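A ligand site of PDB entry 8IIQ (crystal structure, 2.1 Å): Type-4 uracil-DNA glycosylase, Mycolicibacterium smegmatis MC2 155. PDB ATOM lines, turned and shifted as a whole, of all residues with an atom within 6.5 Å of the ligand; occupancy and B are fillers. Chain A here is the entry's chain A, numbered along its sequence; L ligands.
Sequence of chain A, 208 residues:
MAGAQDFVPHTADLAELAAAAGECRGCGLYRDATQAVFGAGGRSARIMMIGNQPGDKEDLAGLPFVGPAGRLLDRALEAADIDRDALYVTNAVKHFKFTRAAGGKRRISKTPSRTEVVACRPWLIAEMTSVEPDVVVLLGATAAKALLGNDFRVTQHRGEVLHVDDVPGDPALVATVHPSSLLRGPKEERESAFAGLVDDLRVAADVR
The backbone NH of Gly 26 lies close to a sulfur (S1) of the ligand. N of Cys 27 sits close to S1 of the ligand (3.6 Å). A sulfur (S3) of the ligand sits close to the backbone NH (N) of His 95 (3.7 Å). FE4 of the ligand is bound by ND1 of His 95 (2.3 Å). NE1 of Trp 123 lies close to S2 of the ligand (3.7 Å). SG of Cys 120 is bound to FE1 of the ligand (2.3 Å). The side-chain sulfur (SG) of Cys 27 is bound to an iron atom (FE2) of the ligand, at 2.3 Å. FE3 of the ligand is bound by SG of Cys 24 (2.3 Å).
The backbone NH (N) of Lys 94 lies close to the side-chain sulfur (SG) of Cys 120 (3.5 Å). NE1 of Trp 123 lies close to SG of Cys 24 (3.3 Å). The side-chain sulfur (SG) of Cys 27 lies close to the backbone NH (N) of Leu 29 (3.5 Å). NE2 of His 95 is in hydrogen-bond range of N of Ala 36. The backbone NH of Ala 4 lies within hydrogen-bond range of the backbone carbonyl oxygen of Ala 119 (2.8 Å). The side-chain sulfur (SG) of Cys 120 lies close to the backbone carbonyl oxygen (O) of Ala 92 (3.8 Å). The side-chain sulfur of Cys 24 sits close to the backbone NH of Gly 26, 3.2 Å away.
Merely in contact with the ligand: Ala 4, Leu 29, Tyr 30, Lys 94 and Ala 119.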
ATOM      1  N   GLY A   3      -7.603  15.443  14.993  1.00  0.00           N
ATOM      2  CA  GLY A   3      -8.587  14.922  15.932  1.00  0.00           C
ATOM      3  C   GLY A   3      -7.945  14.287  17.155  1.00  0.00           C
ATOM      4  O   GLY A   3      -6.918  14.761  17.663  1.00  0.00           O
ATOM      5  N   ALA A   4      -8.536  13.177  17.605  1.00  0.00           N
ATOM      6  CA  ALA A   4      -8.072  12.435  18.764  1.00  0.00           C
ATOM      7  C   ALA A   4      -6.897  11.485  18.465  1.00  0.00           C
ATOM      8  O   ALA A   4      -6.450  10.799  19.375  1.00  0.00           O
ATOM      9  CB  ALA A   4      -9.234  11.617  19.364  1.00  0.00           C
ATOM     10  N   PHE A   7      -3.878  10.950  20.653  1.00  0.00           N
ATOM     11  CA  PHE A   7      -4.148  10.540  22.027  1.00  0.00           C
ATOM     12  C   PHE A   7      -4.391   9.041  22.159  1.00  0.00           C
ATOM     13  O   PHE A   7      -4.305   8.528  23.279  1.00  0.00           O
ATOM     14  CB  PHE A   7      -5.339  11.336  22.589  1.00  0.00           C
ATOM     15  CG  PHE A   7      -5.066  12.793  22.722  1.00  0.00           C
ATOM     16  CD1 PHE A   7      -4.272  13.271  23.768  1.00  0.00           C
ATOM     17  CD2 PHE A   7      -5.547  13.697  21.786  1.00  0.00           C
ATOM     18  CE1 PHE A   7      -4.011  14.640  23.888  1.00  0.00           C
ATOM     19  CE2 PHE A   7      -5.267  15.061  21.896  1.00  0.00           C
ATOM     20  CZ  PHE A   7      -4.495  15.529  22.937  1.00  0.00           C
ATOM     21  N   ALA A  21      -8.302   7.590  26.956  1.00  0.00           N
ATOM     22  CA  ALA A  21      -9.371   8.490  26.543  1.00  0.00           C
ATOM     23  C   ALA A  21      -9.678   9.512  27.623  1.00  0.00           C
ATOM     24  O   ALA A  21     -10.055  10.647  27.310  1.00  0.00           O
ATOM     25  CB  ALA A  21     -10.614   7.697  26.150  1.00  0.00           C
ATOM     26  N   CYS A  24      -7.916  12.570  26.531  1.00  0.00           N
ATOM     27  CA  CYS A  24      -8.055  13.083  25.173  1.00  0.00           C
ATOM     28  C   CYS A  24      -8.431  14.565  25.201  1.00  0.00           C
ATOM     29  O   CYS A  24      -9.274  14.986  25.990  1.00  0.00           O
ATOM     30  CB  CYS A  24      -9.124  12.306  24.409  1.00  0.00           C
ATOM     31  SG  CYS A  24      -9.257  12.728  22.658  1.00  0.00           S
ATOM     32  N   ARG A  25      -7.803  15.351  24.336  1.00  0.00           N
ATOM     33  CA  ARG A  25      -8.260  16.716  24.082  1.00  0.00           C
ATOM     34  C   ARG A  25      -8.570  16.890  22.608  1.00  0.00           C
ATOM     35  O   ARG A  25      -8.469  17.992  22.070  1.00  0.00           O
ATOM     36  CB  ARG A  25      -7.235  17.744  24.568  1.00  0.00           C
ATOM     37  CG  ARG A  25      -6.748  17.471  25.994  1.00  0.00           C
ATOM     38  CD  ARG A  25      -5.935  18.602  26.593  1.00  0.00           C
ATOM     39  NE  ARG A  25      -4.841  19.020  25.697  1.00  0.00           N
ATOM     40  CZ  ARG A  25      -3.755  18.305  25.435  1.00  0.00           C
ATOM     41  NH1 ARG A  25      -3.527  17.142  26.025  1.00  0.00           N
ATOM     42  NH2 ARG A  25      -2.875  18.772  24.555  1.00  0.00           N
ATOM     43  N   GLY A  26      -8.976  15.799  21.947  1.00  0.00           N
ATOM     44  CA  GLY A  26      -9.057  15.702  20.497  1.00  0.00           C
ATOM     45  C   GLY A  26     -10.091  16.591  19.841  1.00  0.00           C
ATOM     46  O   GLY A  26     -10.047  16.746  18.614  1.00  0.00           O
ATOM     47  N   CYS A  27     -11.008  17.142  20.616  1.00  0.00           N
ATOM     48  CA  CYS A  27     -11.885  18.222  20.168  1.00  0.00           C
ATOM     49  C   CYS A  27     -12.217  19.056  21.406  1.00  0.00           C
ATOM     50  O   CYS A  27     -11.619  18.851  22.472  1.00  0.00           O
ATOM     51  CB  CYS A  27     -13.126  17.661  19.456  1.00  0.00           C
ATOM     52  SG  CYS A  27     -14.334  16.891  20.562  1.00  0.00           S
ATOM     53  N   GLY A  28     -13.133  20.004  21.280  1.00  0.00           N
ATOM     54  CA  GLY A  28     -13.416  20.858  22.433  1.00  0.00           C
ATOM     55  C   GLY A  28     -14.262  20.240  23.540  1.00  0.00           C
ATOM     56  O   GLY A  28     -14.322  20.801  24.651  1.00  0.00           O
ATOM     57  N   LEU A  29     -14.876  19.087  23.288  1.00  0.00           N
ATOM     58  CA  LEU A  29     -15.949  18.609  24.169  1.00  0.00           C
ATOM     59  C   LEU A  29     -15.452  18.194  25.556  1.00  0.00           C
ATOM     60  O   LEU A  29     -16.251  18.182  26.492  1.00  0.00           O
ATOM     61  CB  LEU A  29     -16.679  17.435  23.502  1.00  0.00           C
ATOM     62  CG  LEU A  29     -17.524  17.827  22.283  1.00  0.00           C
ATOM     63  CD1 LEU A  29     -18.172  16.601  21.583  1.00  0.00           C
ATOM     64  CD2 LEU A  29     -18.579  18.867  22.732  1.00  0.00           C
ATOM     65  N   TYR A  30     -14.177  17.826  25.723  1.00  0.00           N
ATOM     66  CA  TYR A  30     -13.617  17.451  27.059  1.00  0.00           C
ATOM     67  C   TYR A  30     -13.729  18.601  28.078  1.00  0.00           C
ATOM     68  O   TYR A  30     -13.752  18.306  29.275  1.00  0.00           O
ATOM     69  CB  TYR A  30     -12.154  17.013  26.956  1.00  0.00           C
ATOM     70  CG  TYR A  30     -11.179  18.161  26.805  1.00  0.00           C
ATOM     71  CD1 TYR A  30     -10.985  18.779  25.582  1.00  0.00           C
ATOM     72  CD2 TYR A  30     -10.481  18.655  27.898  1.00  0.00           C
ATOM     73  CE1 TYR A  30     -10.110  19.847  25.446  1.00  0.00           C
ATOM     74  CE2 TYR A  30      -9.605  19.720  27.784  1.00  0.00           C
ATOM     75  CZ  TYR A  30      -9.426  20.313  26.549  1.00  0.00           C
ATOM     76  OH  TYR A  30      -8.563  21.355  26.422  1.00  0.00           O
ATOM     77  N   ARG A  31     -13.817  19.849  27.627  1.00  0.00           N
ATOM     78  CA  ARG A  31     -13.821  21.023  28.533  1.00  0.00           C
ATOM     79  C   ARG A  31     -15.015  21.058  29.513  1.00  0.00           C
ATOM     80  O   ARG A  31     -14.765  21.159  30.713  1.00  0.00           O
ATOM     81  CB  ARG A  31     -13.662  22.309  27.708  1.00  0.00           C
ATOM     82  N   ALA A  36     -14.463  11.612  30.143  1.00  0.00           N
ATOM     83  CA  ALA A  36     -14.731  10.805  28.952  1.00  0.00           C
ATOM     84  C   ALA A  36     -15.522   9.574  29.356  1.00  0.00           C
ATOM     85  O   ALA A  36     -15.310   9.026  30.443  1.00  0.00           O
ATOM     86  CB  ALA A  36     -13.425  10.419  28.256  1.00  0.00           C
ATOM     87  N   ALA A  92     -20.319   7.107  19.466  1.00  0.00           N
ATOM     88  CA  ALA A  92     -19.510   7.726  18.416  1.00  0.00           C
ATOM     89  C   ALA A  92     -18.630   8.856  18.967  1.00  0.00           C
ATOM     90  O   ALA A  92     -17.491   9.036  18.514  1.00  0.00           O
ATOM     91  CB  ALA A  92     -20.443   8.251  17.310  1.00  0.00           C
ATOM     92  N   VAL A  93     -19.127   9.618  19.938  1.00  0.00           N
ATOM     93  CA  VAL A  93     -18.271  10.569  20.644  1.00  0.00           C
ATOM     94  C   VAL A  93     -18.348  10.275  22.142  1.00  0.00           C
ATOM     95  O   VAL A  93     -19.356   9.763  22.627  1.00  0.00           O
ATOM     96  CB  VAL A  93     -18.628  12.035  20.317  1.00  0.00           C
ATOM     97  CG1 VAL A  93     -18.766  12.236  18.786  1.00  0.00           C
ATOM     98  CG2 VAL A  93     -19.863  12.490  21.047  1.00  0.00           C
ATOM     99  N   LYS A  94     -17.253  10.568  22.860  1.00  0.00           N
ATOM    100  CA  LYS A  94     -17.070  10.071  24.219  1.00  0.00           C
ATOM    101  C   LYS A  94     -17.198  11.148  25.296  1.00  0.00           C
ATOM    102  O   LYS A  94     -17.167  10.808  26.470  1.00  0.00           O
ATOM    103  CB  LYS A  94     -15.719   9.359  24.365  1.00  0.00           C
ATOM    104  CG  LYS A  94     -15.415   8.336  23.253  1.00  0.00           C
ATOM    105  CD  LYS A  94     -15.828   6.914  23.620  1.00  0.00           C
ATOM    106  CE  LYS A  94     -15.247   5.850  22.665  1.00  0.00           C
ATOM    107  NZ  LYS A  94     -15.968   5.672  21.334  1.00  0.00           N
ATOM    108  N   HIS A  95     -17.396  12.396  24.876  1.00  0.00           N
ATOM    109  CA  HIS A  95     -17.635  13.524  25.820  1.00  0.00           C
ATOM    110  C   HIS A  95     -19.055  14.106  25.639  1.00  0.00           C
ATOM    111  O   HIS A  95     -19.420  14.415  24.517  1.00  0.00           O
ATOM    112  CB  HIS A  95     -16.508  14.551  25.768  1.00  0.00           C
ATOM    113  CG  HIS A  95     -15.364  14.274  26.668  1.00  0.00           C
ATOM    114  ND1 HIS A  95     -14.159  13.868  26.199  1.00  0.00           N
ATOM    115  CD2 HIS A  95     -15.229  14.367  27.997  1.00  0.00           C
ATOM    116  CE1 HIS A  95     -13.317  13.715  27.182  1.00  0.00           C
ATOM    117  NE2 HIS A  95     -13.956  14.018  28.285  1.00  0.00           N
ATOM    118  N   PHE A  96     -19.802  14.202  26.725  1.00  0.00           N
ATOM    119  CA  PHE A  96     -21.157  14.747  26.709  1.00  0.00           C
ATOM    120  C   PHE A  96     -21.143  16.192  26.183  1.00  0.00           C
ATOM    121  O   PHE A  96     -20.468  17.060  26.744  1.00  0.00           O
ATOM    122  CB  PHE A  96     -21.703  14.681  28.134  1.00  0.00           C
ATOM    123  CG  PHE A  96     -23.151  15.130  28.306  1.00  0.00           C
ATOM    124  CD1 PHE A  96     -24.117  14.843  27.362  1.00  0.00           C
ATOM    125  CD2 PHE A  96     -23.537  15.815  29.461  1.00  0.00           C
ATOM    126  CE1 PHE A  96     -25.451  15.238  27.540  1.00  0.00           C
ATOM    127  CE2 PHE A  96     -24.869  16.207  29.661  1.00  0.00           C
ATOM    128  CZ  PHE A  96     -25.826  15.922  28.695  1.00  0.00           C
ATOM    129  N   GLU A 116     -16.711  17.009  15.195  1.00  0.00           N
ATOM    130  CA  GLU A 116     -16.496  16.327  16.453  1.00  0.00           C
ATOM    131  C   GLU A 116     -16.587  14.821  16.266  1.00  0.00           C
ATOM    132  O   GLU A 116     -15.802  14.066  16.860  1.00  0.00           O
ATOM    133  CB  GLU A 116     -17.519  16.818  17.489  1.00  0.00           C
ATOM    134  CG  GLU A 116     -17.240  18.288  17.881  1.00  0.00           C
ATOM    135  CD  GLU A 116     -18.437  19.008  18.500  1.00  0.00           C
ATOM    136  OE1 GLU A 116     -19.592  18.584  18.316  1.00  0.00           O
ATOM    137  OE2 GLU A 116     -18.211  20.023  19.193  1.00  0.00           O
ATOM    138  N   ALA A 119     -13.400  13.828  14.627  1.00  0.00           N
ATOM    139  CA  ALA A 119     -12.288  13.985  15.578  1.00  0.00           C
ATOM    140  C   ALA A 119     -12.188  12.784  16.520  1.00  0.00           C
ATOM    141  O   ALA A 119     -11.090  12.314  16.832  1.00  0.00           O
ATOM    142  CB  ALA A 119     -12.475  15.259  16.406  1.00  0.00           C
ATOM    143  N   CYS A 120     -13.337  12.281  16.984  1.00  0.00           N
ATOM    144  CA  CYS A 120     -13.411  11.204  17.955  1.00  0.00           C
ATOM    145  C   CYS A 120     -13.378   9.822  17.325  1.00  0.00           C
ATOM    146  O   CYS A 120     -13.161   8.833  18.049  1.00  0.00           O
ATOM    147  CB  CYS A 120     -14.699  11.350  18.791  1.00  0.00           C
ATOM    148  SG  CYS A 120     -14.660  10.548  20.454  1.00  0.00           S
ATOM    149  N   ARG A 121     -13.593   9.730  16.003  1.00  0.00           N
ATOM    150  CA  ARG A 121     -13.653   8.423  15.347  1.00  0.00           C
ATOM    151  C   ARG A 121     -12.439   7.539  15.603  1.00  0.00           C
ATOM    152  O   ARG A 121     -12.621   6.310  15.673  1.00  0.00           O
ATOM    153  CB  ARG A 121     -13.856   8.583  13.835  1.00  0.00           C
ATOM    154  CG  ARG A 121     -14.255   7.246  13.137  1.00  0.00           C
ATOM    155  CD  ARG A 121     -14.950   7.447  11.776  1.00  0.00           C
ATOM    156  NE  ARG A 121     -14.133   8.289  10.916  1.00  0.00           N
ATOM    157  CZ  ARG A 121     -14.592   8.945   9.848  1.00  0.00           C
ATOM    158  NH1 ARG A 121     -15.853   8.808   9.443  1.00  0.00           N
ATOM    159  NH2 ARG A 121     -13.778   9.759   9.188  1.00  0.00           N
ATOM    160  N   TRP A 123     -11.018   6.745  18.335  1.00  0.00           N
ATOM    161  CA  TRP A 123     -11.357   5.894  19.479  1.00  0.00           C
ATOM    162  C   TRP A 123     -12.253   4.748  19.030  1.00  0.00           C
ATOM    163  O   TRP A 123     -12.020   3.581  19.357  1.00  0.00           O
ATOM    164  CB  TRP A 123     -12.040   6.719  20.575  1.00  0.00           C
ATOM    165  CG  TRP A 123     -11.102   7.694  21.255  1.00  0.00           C
ATOM    166  CD1 TRP A 123     -11.189   9.076  21.267  1.00  0.00           C
ATOM    167  CD2 TRP A 123      -9.924   7.351  22.004  1.00  0.00           C
ATOM    168  NE1 TRP A 123     -10.125   9.602  21.975  1.00  0.00           N
ATOM    169  CE2 TRP A 123      -9.333   8.565  22.428  1.00  0.00           C
ATOM    170  CE3 TRP A 123      -9.313   6.136  22.341  1.00  0.00           C
ATOM    171  CZ2 TRP A 123      -8.168   8.590  23.195  1.00  0.00           C
ATOM    172  CZ3 TRP A 123      -8.147   6.168  23.096  1.00  0.00           C
ATOM    173  CH2 TRP A 123      -7.586   7.386  23.522  1.00  0.00           C
HETATM  174 FE1  LIG L   1     -13.789  12.310  21.591  1.00  0.00          FE
HETATM  175 FE2  LIG L   1     -13.446  15.036  21.546  1.00  0.00          FE
HETATM  176 FE3  LIG L   1     -11.458  13.412  22.530  1.00  0.00          FE
HETATM  177 FE4  LIG L   1     -13.809  13.703  23.927  1.00  0.00          FE
HETATM  178  S1  LIG L   1     -12.263  15.342  23.467  1.00  0.00           S
HETATM  179  S2  LIG L   1     -12.715  11.759  23.516  1.00  0.00           S
HETATM  180  S3  LIG L   1     -15.335  13.865  22.214  1.00  0.00           S
HETATM  181  S4  LIG L   1     -12.236  13.523  20.403  1.00  0.00           S
